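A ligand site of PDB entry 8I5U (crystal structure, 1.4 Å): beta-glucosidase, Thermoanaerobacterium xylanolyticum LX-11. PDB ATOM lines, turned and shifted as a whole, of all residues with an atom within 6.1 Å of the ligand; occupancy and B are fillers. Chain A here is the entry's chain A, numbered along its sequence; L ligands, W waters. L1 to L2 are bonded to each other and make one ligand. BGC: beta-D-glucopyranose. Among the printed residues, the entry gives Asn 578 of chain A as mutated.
An oxygen (O6) of BGC L2 is in hydrogen-bond range of the side-chain carboxylate of Glu 762.
O3 of BGC L2 is in hydrogen-bond range of OD2 of Asp 437, 2.7 Å away.
O3 of BGC L2 lies within hydrogen-bond range of NE2 of His 492, at 2.8 Å.
An oxygen (O4) of BGC L2 is in hydrogen-bond range of the backbone carbonyl oxygen (O) of Thr 576 (2.8 Å).
OG1 of Thr 576 sits at hydrogen-bond distance from O4 of BGC L2, at 2.8 Å.
NH1 of Arg 771 sits at hydrogen-bond distance from O6 of BGC L2 (2.8 Å).
The side-chain carboxylate (OE2) of Glu 426 is in hydrogen-bond range of an oxygen (O2) of BGC L2 (2.9 Å).
NH2 of Arg 777 lies within hydrogen-bond range of O4 of BGC L2 (3.0 Å).
ND2 of Asn 578 lies within hydrogen-bond range of O3 of BGC L1.
An oxygen (O6) of BGC L1 is in hydrogen-bond range of the indole nitrogen of Trp 510, 3.4 Å away.
O4 of BGC L1 sits at hydrogen-bond distance from OH of Tyr 430 (3.4 Å).
O of Arg 771 lies within hydrogen-bond range of N of Glu 762, 3.3 Å away.
The guanidinium group (NE) of Arg 777 is in salt-bridge range of the side-chain carboxylate (OE1) of Glu 762.
The side-chain carboxylate (OD2) of Asp 437 sits at hydrogen-bond distance from the side-chain hydroxyl (OG1) of Thr 576, 2.7 Å away.
The side-chain carboxylate (OE2) of Glu 715 lies within salt-bridge range of the guanidinium group (NE) of Arg 771, at 2.9 Å.
The backbone NH of Glu 426 is in hydrogen-bond range of the backbone carbonyl oxygen of Tyr 432, at 2.8 Å.
The side-chain hydroxyl (OH) of Tyr 775 is in hydrogen-bond range of the side-chain carboxylate (OE2) of Glu 426 (2.7 Å).
OH of Tyr 430 lies within hydrogen-bond range of OH of Tyr 47, at 2.8 Å.
The backbone carbonyl oxygen of Tyr 577 lies close to the side-chain amide oxygen of Gln 712 (3.3 Å).
Water W2 lies within hydrogen-bond range of an oxygen (O6) of BGC L1 (2.7 Å) and the indole nitrogen of Trp 510 (3.3 Å).
Water W4 lies within hydrogen-bond range of OD1 of Asn 578 (2.7 Å), O4 of BGC L1 (2.7 Å) and NE2 of Gln 712 (3.4 Å).
Water W5 lies within hydrogen-bond range of the side-chain hydroxyl of Tyr 432, an oxygen (O1) of BGC L1, the backbone NH of Trp 510 and the backbone NH of Asp 509.
Water W1 lies within hydrogen-bond range of OH of Tyr 47 and O4 of BGC L1.
OH of Tyr 47 touches C6 of BGC L1, 3.6 Å away.
CE2 of Tyr 432 touches O2 of BGC L1 (3.4 Å).
Thr 435 touches the ligand.
CE1 of Tyr 508 touches O2 of BGC L1, 3.4 Å away.
CH2 of Trp 516 touches O3 of BGC L2, 3.6 Å away.
NE2 of Gln 712 touches C6 of BGC L2, at 3.8 Å.
CH2 of Trp 717 touches C6 of BGC L2, at 3.5 Å.
OH of Tyr 775 touches C5 of BGC L2, at 3.7 Å.
Hydrophobic or aromatic side chains within 4 Å of the ligand: Tyr 47, Tyr 430, Tyr 432, His 492, Tyr 508, Trp 510, Trp 516 and Trp 717.
Within 4 Å of the ligand: Tyr 47, Glu 426, Tyr 430, Tyr 432, Thr 435, Asp 437, His 492, Tyr 508, Trp 510, Trp 516, Thr 576, Asn 578, Gln 712, Trp 717, Glu 762, Arg 771, Tyr 775 and Arg 777.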
ATOM      1  N   TYR A  47     -35.039  17.928 -21.756  1.00  0.00           N
ATOM      2  CA  TYR A  47     -35.359  19.278 -21.281  1.00  0.00           C
ATOM      3  C   TYR A  47     -34.340  20.311 -21.828  1.00  0.00           C
ATOM      4  O   TYR A  47     -33.232  19.929 -22.182  1.00  0.00           O
ATOM      5  CB  TYR A  47     -35.416  19.315 -19.743  1.00  0.00           C
ATOM      6  CG  TYR A  47     -34.160  18.808 -18.999  1.00  0.00           C
ATOM      7  CD1 TYR A  47     -33.124  19.682 -18.656  1.00  0.00           C
ATOM      8  CD2 TYR A  47     -34.028  17.455 -18.619  1.00  0.00           C
ATOM      9  CE1 TYR A  47     -31.997  19.237 -17.978  1.00  0.00           C
ATOM     10  CE2 TYR A  47     -32.893  17.006 -17.921  1.00  0.00           C
ATOM     11  CZ  TYR A  47     -31.868  17.894 -17.615  1.00  0.00           C
ATOM     12  OH  TYR A  47     -30.721  17.481 -16.920  1.00  0.00           O
ATOM     13  N   GLU A 426     -21.999  24.506  -9.061  1.00  0.00           N
ATOM     14  CA  GLU A 426     -22.082  23.155  -9.611  1.00  0.00           C
ATOM     15  C   GLU A 426     -21.960  23.211 -11.134  1.00  0.00           C
ATOM     16  O   GLU A 426     -21.156  22.506 -11.736  1.00  0.00           O
ATOM     17  CB  GLU A 426     -23.429  22.525  -9.182  1.00  0.00           C
ATOM     18  CG  GLU A 426     -23.644  21.104  -9.655  1.00  0.00           C
ATOM     19  CD  GLU A 426     -24.989  20.525  -9.241  1.00  0.00           C
ATOM     20  OE1 GLU A 426     -25.578  20.958  -8.240  1.00  0.00           O
ATOM     21  OE2 GLU A 426     -25.402  19.587  -9.927  1.00  0.00           O
ATOM     22  N   ASP A 429     -26.556  25.201 -15.628  1.00  0.00           N
ATOM     23  CA  ASP A 429     -27.861  24.561 -15.787  1.00  0.00           C
ATOM     24  C   ASP A 429     -28.487  24.251 -14.448  1.00  0.00           C
ATOM     25  O   ASP A 429     -29.711  24.309 -14.305  1.00  0.00           O
ATOM     26  CB  ASP A 429     -27.736  23.269 -16.583  1.00  0.00           C
ATOM     27  CG  ASP A 429     -27.381  23.493 -18.039  1.00  0.00           C
ATOM     28  OD1 ASP A 429     -28.266  23.851 -18.832  1.00  0.00           O
ATOM     29  OD2 ASP A 429     -26.217  23.294 -18.416  1.00  0.00           O
ATOM     30  N   TYR A 430     -27.646  23.871 -13.488  1.00  0.00           N
ATOM     31  CA  TYR A 430     -28.053  23.485 -12.149  1.00  0.00           C
ATOM     32  C   TYR A 430     -27.347  24.490 -11.230  1.00  0.00           C
ATOM     33  O   TYR A 430     -26.240  24.240 -10.748  1.00  0.00           O
ATOM     34  CB  TYR A 430     -27.607  22.048 -11.831  1.00  0.00           C
ATOM     35  CG  TYR A 430     -27.777  20.979 -12.882  1.00  0.00           C
ATOM     36  CD1 TYR A 430     -28.790  21.004 -13.842  1.00  0.00           C
ATOM     37  CD2 TYR A 430     -26.942  19.866 -12.890  1.00  0.00           C
ATOM     38  CE1 TYR A 430     -28.928  19.979 -14.776  1.00  0.00           C
ATOM     39  CE2 TYR A 430     -27.072  18.843 -13.811  1.00  0.00           C
ATOM     40  CZ  TYR A 430     -28.078  18.893 -14.745  1.00  0.00           C
ATOM     41  OH  TYR A 430     -28.215  17.875 -15.662  1.00  0.00           O
ATOM     42  N   ASN A 431     -27.988  25.641 -11.031  1.00  0.00           N
ATOM     43  CA  ASN A 431     -27.325  26.853 -10.558  1.00  0.00           C
ATOM     44  C   ASN A 431     -27.269  26.886  -9.035  1.00  0.00           C
ATOM     45  O   ASN A 431     -28.020  27.611  -8.367  1.00  0.00           O
ATOM     46  CB  ASN A 431     -28.055  28.072 -11.133  1.00  0.00           C
ATOM     47  CG  ASN A 431     -27.223  29.341 -11.091  1.00  0.00           C
ATOM     48  OD1 ASN A 431     -27.130  29.985 -10.069  1.00  0.00           O
ATOM     49  ND2 ASN A 431     -26.630  29.690 -12.225  1.00  0.00           N
ATOM     50  N   TYR A 432     -26.405  26.066  -8.465  1.00  0.00           N
ATOM     51  CA  TYR A 432     -26.282  25.897  -7.014  1.00  0.00           C
ATOM     52  C   TYR A 432     -24.827  26.058  -6.612  1.00  0.00           C
ATOM     53  O   TYR A 432     -23.941  25.468  -7.247  1.00  0.00           O
ATOM     54  CB  TYR A 432     -26.784  24.497  -6.595  1.00  0.00           C
ATOM     55  CG  TYR A 432     -28.188  24.247  -7.081  1.00  0.00           C
ATOM     56  CD1 TYR A 432     -29.197  25.094  -6.640  1.00  0.00           C
ATOM     57  CD2 TYR A 432     -28.517  23.243  -7.992  1.00  0.00           C
ATOM     58  CE1 TYR A 432     -30.498  24.961  -7.053  1.00  0.00           C
ATOM     59  CE2 TYR A 432     -29.841  23.113  -8.425  1.00  0.00           C
ATOM     60  CZ  TYR A 432     -30.802  24.001  -7.953  1.00  0.00           C
ATOM     61  OH  TYR A 432     -32.150  23.936  -8.343  1.00  0.00           O
ATOM     62  N   THR A 435     -22.244  22.700  -4.380  1.00  0.00           N
ATOM     63  CA  THR A 435     -22.964  21.460  -4.193  1.00  0.00           C
ATOM     64  C   THR A 435     -22.039  20.409  -3.595  1.00  0.00           C
ATOM     65  O   THR A 435     -21.026  20.032  -4.218  1.00  0.00           O
ATOM     66  CB  THR A 435     -23.550  20.987  -5.505  1.00  0.00           C
ATOM     67  OG1 THR A 435     -24.502  21.970  -5.942  1.00  0.00           O
ATOM     68  CG2 THR A 435     -24.238  19.652  -5.379  1.00  0.00           C
ATOM     69  N   ASP A 437     -22.088  17.136  -2.584  1.00  0.00           N
ATOM     70  CA  ASP A 437     -21.882  15.800  -3.156  1.00  0.00           C
ATOM     71  C   ASP A 437     -20.996  15.852  -4.398  1.00  0.00           C
ATOM     72  O   ASP A 437     -20.403  14.832  -4.759  1.00  0.00           O
ATOM     73  CB  ASP A 437     -23.228  15.125  -3.461  1.00  0.00           C
ATOM     74  CG  ASP A 437     -24.168  15.994  -4.276  1.00  0.00           C
ATOM     75  OD1 ASP A 437     -24.601  17.027  -3.724  1.00  0.00           O
ATOM     76  OD2 ASP A 437     -24.475  15.646  -5.412  1.00  0.00           O
ATOM     77  N   VAL A 438     -20.981  17.002  -5.072  1.00  0.00           N
ATOM     78  CA  VAL A 438     -20.137  17.280  -6.253  1.00  0.00           C
ATOM     79  C   VAL A 438     -18.756  17.785  -5.832  1.00  0.00           C
ATOM     80  O   VAL A 438     -17.735  17.331  -6.409  1.00  0.00           O
ATOM     81  CB  VAL A 438     -20.845  18.276  -7.191  1.00  0.00           C
ATOM     82  CG1 VAL A 438     -19.965  18.632  -8.387  1.00  0.00           C
ATOM     83  CG2 VAL A 438     -22.176  17.719  -7.673  1.00  0.00           C
ATOM     84  N   HIS A 492     -27.331  20.213   0.661  1.00  0.00           N
ATOM     85  CA  HIS A 492     -26.906  19.954  -0.711  1.00  0.00           C
ATOM     86  C   HIS A 492     -26.036  21.079  -1.256  1.00  0.00           C
ATOM     87  O   HIS A 492     -25.071  20.805  -1.953  1.00  0.00           O
ATOM     88  CB  HIS A 492     -28.127  19.788  -1.589  1.00  0.00           C
ATOM     89  CG  HIS A 492     -27.838  19.559  -3.046  1.00  0.00           C
ATOM     90  ND1 HIS A 492     -27.808  20.585  -3.962  1.00  0.00           N
ATOM     91  CD2 HIS A 492     -27.626  18.419  -3.745  1.00  0.00           C
ATOM     92  CE1 HIS A 492     -27.582  20.095  -5.160  1.00  0.00           C
ATOM     93  NE2 HIS A 492     -27.457  18.782  -5.061  1.00  0.00           N
ATOM     94  N   TYR A 508     -31.477  23.703  -4.068  1.00  0.00           N
ATOM     95  CA  TYR A 508     -31.900  22.502  -4.760  1.00  0.00           C
ATOM     96  C   TYR A 508     -33.188  21.985  -4.161  1.00  0.00           C
ATOM     97  O   TYR A 508     -33.256  21.687  -2.970  1.00  0.00           O
ATOM     98  CB  TYR A 508     -30.788  21.438  -4.615  1.00  0.00           C
ATOM     99  CG  TYR A 508     -31.057  20.082  -5.195  1.00  0.00           C
ATOM    100  CD1 TYR A 508     -30.822  19.809  -6.543  1.00  0.00           C
ATOM    101  CD2 TYR A 508     -31.446  19.017  -4.370  1.00  0.00           C
ATOM    102  CE1 TYR A 508     -31.023  18.538  -7.067  1.00  0.00           C
ATOM    103  CE2 TYR A 508     -31.631  17.741  -4.887  1.00  0.00           C
ATOM    104  CZ  TYR A 508     -31.427  17.501  -6.235  1.00  0.00           C
ATOM    105  OH  TYR A 508     -31.596  16.252  -6.808  1.00  0.00           O
ATOM    106  N   ASP A 509     -34.199  21.878  -5.015  1.00  0.00           N
ATOM    107  CA  ASP A 509     -35.529  21.399  -4.588  1.00  0.00           C
ATOM    108  C   ASP A 509     -36.087  20.266  -5.437  1.00  0.00           C
ATOM    109  O   ASP A 509     -37.240  19.874  -5.248  1.00  0.00           O
ATOM    110  CB  ASP A 509     -36.529  22.573  -4.514  1.00  0.00           C
ATOM    111  CG  ASP A 509     -36.782  23.249  -5.850  1.00  0.00           C
ATOM    112  OD1 ASP A 509     -36.166  22.905  -6.871  1.00  0.00           O
ATOM    113  OD2 ASP A 509     -37.648  24.160  -5.893  1.00  0.00           O
ATOM    114  N   TRP A 510     -35.309  19.736  -6.365  1.00  0.00           N
ATOM    115  CA  TRP A 510     -35.784  18.633  -7.204  1.00  0.00           C
ATOM    116  C   TRP A 510     -36.065  17.386  -6.361  1.00  0.00           C
ATOM    117  O   TRP A 510     -36.971  16.618  -6.665  1.00  0.00           O
ATOM    118  CB  TRP A 510     -34.771  18.331  -8.312  1.00  0.00           C
ATOM    119  CG  TRP A 510     -35.240  17.317  -9.309  1.00  0.00           C
ATOM    120  CD1 TRP A 510     -34.670  16.110  -9.582  1.00  0.00           C
ATOM    121  CD2 TRP A 510     -36.388  17.419 -10.172  1.00  0.00           C
ATOM    122  NE1 TRP A 510     -35.391  15.449 -10.547  1.00  0.00           N
ATOM    123  CE2 TRP A 510     -36.440  16.237 -10.940  1.00  0.00           C
ATOM    124  CE3 TRP A 510     -37.369  18.397 -10.385  1.00  0.00           C
ATOM    125  CZ2 TRP A 510     -37.438  15.979 -11.887  1.00  0.00           C
ATOM    126  CZ3 TRP A 510     -38.377  18.155 -11.344  1.00  0.00           C
ATOM    127  CH2 TRP A 510     -38.397  16.954 -12.080  1.00  0.00           C
ATOM    128  N   TRP A 516     -30.522  12.481   2.122  1.00  0.00           N
ATOM    129  CA  TRP A 516     -29.409  11.878   1.372  1.00  0.00           C
ATOM    130  C   TRP A 516     -28.458  11.170   2.332  1.00  0.00           C
ATOM    131  O   TRP A 516     -28.303  11.565   3.477  1.00  0.00           O
ATOM    132  CB  TRP A 516     -28.686  12.897   0.494  1.00  0.00           C
ATOM    133  CG  TRP A 516     -29.435  13.238  -0.760  1.00  0.00           C
ATOM    134  CD1 TRP A 516     -30.784  13.124  -0.991  1.00  0.00           C
ATOM    135  CD2 TRP A 516     -28.875  13.777  -1.962  1.00  0.00           C
ATOM    136  NE1 TRP A 516     -31.085  13.547  -2.243  1.00  0.00           N
ATOM    137  CE2 TRP A 516     -29.932  13.946  -2.876  1.00  0.00           C
ATOM    138  CE3 TRP A 516     -27.574  14.104  -2.360  1.00  0.00           C
ATOM    139  CZ2 TRP A 516     -29.736  14.452  -4.165  1.00  0.00           C
ATOM    140  CZ3 TRP A 516     -27.379  14.609  -3.650  1.00  0.00           C
ATOM    141  CH2 TRP A 516     -28.440  14.781  -4.527  1.00  0.00           C
ATOM    142  N   GLN A 575     -28.705  10.061  -2.991  1.00  0.00           N
ATOM    143  CA  GLN A 575     -27.280  10.356  -3.034  1.00  0.00           C
ATOM    144  C   GLN A 575     -26.956  10.977  -4.396  1.00  0.00           C
ATOM    145  O   GLN A 575     -27.840  11.176  -5.240  1.00  0.00           O
ATOM    146  CB  GLN A 575     -26.429   9.112  -2.723  1.00  0.00           C
ATOM    147  CG  GLN A 575     -26.964   7.776  -3.216  1.00  0.00           C
ATOM    148  CD  GLN A 575     -26.986   7.683  -4.720  1.00  0.00           C
ATOM    149  OE1 GLN A 575     -26.049   8.093  -5.382  1.00  0.00           O
ATOM    150  NE2 GLN A 575     -28.045   7.137  -5.272  1.00  0.00           N
ATOM    151  N   THR A 576     -25.673  11.294  -4.646  1.00  0.00           N
ATOM    152  CA  THR A 576     -25.265  12.096  -5.811  1.00  0.00           C
ATOM    153  C   THR A 576     -25.718  11.532  -7.158  1.00  0.00           C
ATOM    154  O   THR A 576     -25.961  12.291  -8.104  1.00  0.00           O
ATOM    155  CB  THR A 576     -23.719  12.321  -5.815  1.00  0.00           C
ATOM    156  OG1 THR A 576     -23.393  13.501  -6.587  1.00  0.00           O
ATOM    157  CG2 THR A 576     -22.953  11.112  -6.370  1.00  0.00           C
ATOM    158  N   TYR A 577     -25.825  10.207  -7.254  1.00  0.00           N
ATOM    159  CA  TYR A 577     -26.369   9.558  -8.455  1.00  0.00           C
ATOM    160  C   TYR A 577     -27.877   9.636  -8.280  1.00  0.00           C
ATOM    161  O   TYR A 577     -28.551   8.646  -7.956  1.00  0.00           O
ATOM    162  CB  TYR A 577     -25.875   8.118  -8.627  1.00  0.00           C
ATOM    163  CG  TYR A 577     -24.372   8.016  -8.804  1.00  0.00           C
ATOM    164  CD1 TYR A 577     -23.511   7.946  -7.714  1.00  0.00           C
ATOM    165  CD2 TYR A 577     -23.825   8.010 -10.081  1.00  0.00           C
ATOM    166  CE1 TYR A 577     -22.129   7.847  -7.888  1.00  0.00           C
ATOM    167  CE2 TYR A 577     -22.452   7.921 -10.260  1.00  0.00           C
ATOM    168  CZ  TYR A 577     -21.631   7.831  -9.165  1.00  0.00           C
ATOM    169  OH  TYR A 577     -20.259   7.740  -9.369  1.00  0.00           O
ATOM    170  N   ASN A 578     -28.387  10.834  -8.538  1.00  0.00           N
ATOM    171  CA  ASN A 578     -29.721  11.205  -8.060  1.00  0.00           C
ATOM    172  C   ASN A 578     -30.888  10.713  -8.921  1.00  0.00           C
ATOM    173  O   ASN A 578     -32.020  11.077  -8.634  1.00  0.00           O
ATOM    174  CB  ASN A 578     -29.819  12.720  -7.826  1.00  0.00           C
ATOM    175  CG  ASN A 578     -29.774  13.540  -9.095  1.00  0.00           C
ATOM    176  OD1 ASN A 578     -29.399  13.058 -10.162  1.00  0.00           O
ATOM    177  ND2 ASN A 578     -30.167  14.810  -8.979  1.00  0.00           N
ATOM    178  N   GLN A 712     -28.187   7.210 -15.632  1.00  0.00           N
ATOM    179  CA  GLN A 712     -26.888   7.478 -14.994  1.00  0.00           C
ATOM    180  C   GLN A 712     -25.956   6.278 -15.030  1.00  0.00           C
ATOM    181  O   GLN A 712     -24.759   6.447 -15.113  1.00  0.00           O
ATOM    182  CB  GLN A 712     -27.054   8.002 -13.593  1.00  0.00           C
ATOM    183  CG  GLN A 712     -27.667   9.376 -13.590  1.00  0.00           C
ATOM    184  CD  GLN A 712     -27.913   9.917 -12.206  1.00  0.00           C
ATOM    185  OE1 GLN A 712     -27.989   9.176 -11.215  1.00  0.00           O
ATOM    186  NE2 GLN A 712     -28.064  11.244 -12.128  1.00  0.00           N
ATOM    187  N   GLU A 715     -24.045   6.457 -18.261  1.00  0.00           N
ATOM    188  CA  GLU A 715     -23.222   7.641 -18.459  1.00  0.00           C
ATOM    189  C   GLU A 715     -21.813   7.376 -17.936  1.00  0.00           C
ATOM    190  O   GLU A 715     -21.622   6.685 -16.955  1.00  0.00           O
ATOM    191  CB  GLU A 715     -23.788   8.833 -17.676  1.00  0.00           C
ATOM    192  CG  GLU A 715     -25.062   9.416 -18.289  1.00  0.00           C
ATOM    193  CD  GLU A 715     -25.636  10.595 -17.526  1.00  0.00           C
ATOM    194  OE1 GLU A 715     -25.560  10.613 -16.286  1.00  0.00           O
ATOM    195  OE2 GLU A 715     -26.206  11.508 -18.189  1.00  0.00           O
ATOM    196  N   TRP A 717     -19.219   9.676 -16.082  1.00  0.00           N
ATOM    197  CA  TRP A 717     -19.099  10.948 -15.360  1.00  0.00           C
ATOM    198  C   TRP A 717     -17.628  11.324 -15.358  1.00  0.00           C
ATOM    199  O   TRP A 717     -16.768  10.605 -14.832  1.00  0.00           O
ATOM    200  CB  TRP A 717     -19.659  10.868 -13.947  1.00  0.00           C
ATOM    201  CG  TRP A 717     -21.166  10.823 -13.895  1.00  0.00           C
ATOM    202  CD1 TRP A 717     -22.007  10.572 -14.937  1.00  0.00           C
ATOM    203  CD2 TRP A 717     -21.985  11.043 -12.752  1.00  0.00           C
ATOM    204  NE1 TRP A 717     -23.312  10.613 -14.500  1.00  0.00           N
ATOM    205  CE2 TRP A 717     -23.331  10.918 -13.179  1.00  0.00           C
ATOM    206  CE3 TRP A 717     -21.721  11.366 -11.415  1.00  0.00           C
ATOM    207  CZ2 TRP A 717     -24.418  11.077 -12.304  1.00  0.00           C
ATOM    208  CZ3 TRP A 717     -22.787  11.521 -10.545  1.00  0.00           C
ATOM    209  CH2 TRP A 717     -24.118  11.378 -10.997  1.00  0.00           C
ATOM    210  N   GLU A 762     -20.635  17.275 -16.964  1.00  0.00           N
ATOM    211  CA  GLU A 762     -20.808  16.182 -16.015  1.00  0.00           C
ATOM    212  C   GLU A 762     -20.602  14.845 -16.705  1.00  0.00           C
ATOM    213  O   GLU A 762     -19.821  13.999 -16.248  1.00  0.00           O
ATOM    214  CB  GLU A 762     -22.216  16.218 -15.416  1.00  0.00           C
ATOM    215  CG  GLU A 762     -22.644  14.997 -14.624  1.00  0.00           C
ATOM    216  CD  GLU A 762     -22.221  15.003 -13.169  1.00  0.00           C
ATOM    217  OE1 GLU A 762     -21.019  14.934 -12.881  1.00  0.00           O
ATOM    218  OE2 GLU A 762     -23.097  15.011 -12.280  1.00  0.00           O
ATOM    219  N   ARG A 771     -24.444  15.733 -20.909  1.00  0.00           N
ATOM    220  CA  ARG A 771     -25.350  16.363 -19.976  1.00  0.00           C
ATOM    221  C   ARG A 771     -24.541  17.304 -19.084  1.00  0.00           C
ATOM    222  O   ARG A 771     -23.550  16.890 -18.490  1.00  0.00           O
ATOM    223  CB  ARG A 771     -26.065  15.308 -19.133  1.00  0.00           C
ATOM    224  CG  ARG A 771     -27.024  15.875 -18.116  1.00  0.00           C
ATOM    225  CD  ARG A 771     -27.901  14.769 -17.535  1.00  0.00           C
ATOM    226  NE  ARG A 771     -27.141  13.827 -16.721  1.00  0.00           N
ATOM    227  CZ  ARG A 771     -26.819  14.000 -15.448  1.00  0.00           C
ATOM    228  NH1 ARG A 771     -27.133  15.122 -14.807  1.00  0.00           N
ATOM    229  NH2 ARG A 771     -26.141  13.059 -14.802  1.00  0.00           N
ATOM    230  N   TYR A 775     -19.080  22.005 -15.874  1.00  0.00           N
ATOM    231  CA  TYR A 775     -19.449  21.297 -14.643  1.00  0.00           C
ATOM    232  C   TYR A 775     -18.283  21.251 -13.653  1.00  0.00           C
ATOM    233  O   TYR A 775     -17.134  21.130 -14.063  1.00  0.00           O
ATOM    234  CB  TYR A 775     -19.974  19.872 -14.979  1.00  0.00           C
ATOM    235  CG  TYR A 775     -20.913  19.336 -13.911  1.00  0.00           C
ATOM    236  CD1 TYR A 775     -22.221  19.794 -13.842  1.00  0.00           C
ATOM    237  CD2 TYR A 775     -20.506  18.387 -12.959  1.00  0.00           C
ATOM    238  CE1 TYR A 775     -23.086  19.353 -12.842  1.00  0.00           C
ATOM    239  CE2 TYR A 775     -21.363  17.939 -11.963  1.00  0.00           C
ATOM    240  CZ  TYR A 775     -22.661  18.427 -11.913  1.00  0.00           C
ATOM    241  OH  TYR A 775     -23.474  17.972 -10.902  1.00  0.00           O
ATOM    242  N   ARG A 777     -17.473  18.923 -11.282  1.00  0.00           N
ATOM    243  CA  ARG A 777     -16.920  17.632 -10.897  1.00  0.00           C
ATOM    244  C   ARG A 777     -15.569  17.269 -11.548  1.00  0.00           C
ATOM    245  O   ARG A 777     -14.719  16.746 -10.841  1.00  0.00           O
ATOM    246  CB  ARG A 777     -17.955  16.496 -11.083  1.00  0.00           C
ATOM    247  CG  ARG A 777     -17.865  15.407 -10.018  1.00  0.00           C
ATOM    248  CD  ARG A 777     -18.789  14.197 -10.226  1.00  0.00           C
ATOM    249  NE  ARG A 777     -20.220  14.543 -10.319  1.00  0.00           N
ATOM    250  CZ  ARG A 777     -21.126  14.445  -9.339  1.00  0.00           C
ATOM    251  NH1 ARG A 777     -20.809  14.068  -8.119  1.00  0.00           N
ATOM    252  NH2 ARG A 777     -22.381  14.741  -9.635  1.00  0.00           N
HETATM  253  C2  BGC L   1     -30.755  19.284 -10.692  1.00  0.00           C
HETATM  254  C3  BGC L   1     -29.970  18.184 -11.382  1.00  0.00           C
HETATM  255  C4  BGC L   1     -30.887  17.349 -12.292  1.00  0.00           C
HETATM  256  C5  BGC L   1     -31.762  18.236 -13.185  1.00  0.00           C
HETATM  257  C6  BGC L   1     -32.837  17.499 -13.994  1.00  0.00           C
HETATM  258  C1  BGC L   1     -31.505  20.120 -11.712  1.00  0.00           C
HETATM  259  O1  BGC L   1     -32.254  21.114 -11.009  1.00  0.00           O
HETATM  260  O2  BGC L   1     -29.914  20.100  -9.892  1.00  0.00           O
HETATM  261  O3  BGC L   1     -29.447  17.384 -10.327  1.00  0.00           O
HETATM  262  O4  BGC L   1     -30.066  16.517 -13.104  1.00  0.00           O
HETATM  263  O5  BGC L   1     -32.390  19.234 -12.374  1.00  0.00           O
HETATM  264  O6  BGC L   1     -33.766  16.877 -13.109  1.00  0.00           O
HETATM  265  C2  BGC L   2     -27.743  17.525  -8.667  1.00  0.00           C
HETATM  266  C3  BGC L   2     -26.436  16.891  -8.172  1.00  0.00           C
HETATM  267  C4  BGC L   2     -26.277  15.498  -8.774  1.00  0.00           C
HETATM  268  C5  BGC L   2     -26.323  15.622 -10.296  1.00  0.00           C
HETATM  269  C6  BGC L   2     -26.075  14.331 -11.045  1.00  0.00           C
HETATM  270  C1  BGC L   2     -28.012  17.320 -10.167  1.00  0.00           C
HETATM  271  O2  BGC L   2     -27.761  18.919  -8.327  1.00  0.00           O
HETATM  272  O3  BGC L   2     -26.514  16.826  -6.754  1.00  0.00           O
HETATM  273  O4  BGC L   2     -25.054  14.901  -8.330  1.00  0.00           O
HETATM  274  O5  BGC L   2     -27.649  16.042 -10.662  1.00  0.00           O
HETATM  275  O6  BGC L   2     -25.708  14.561 -12.417  1.00  0.00           O
HETATM  276  O   HOH W   1     -31.019  15.139 -15.935  1.00  0.00           O
HETATM  277  O   HOH W   2     -33.046  14.350 -12.559  1.00  0.00           O
HETATM  278  O   HOH W   3     -35.763  16.143 -15.267  1.00  0.00           O
HETATM  279  O   HOH W   4     -30.206  13.862 -12.587  1.00  0.00           O
HETATM  280  O   HOH W   5     -33.474  21.657  -8.152  1.00  0.00           O
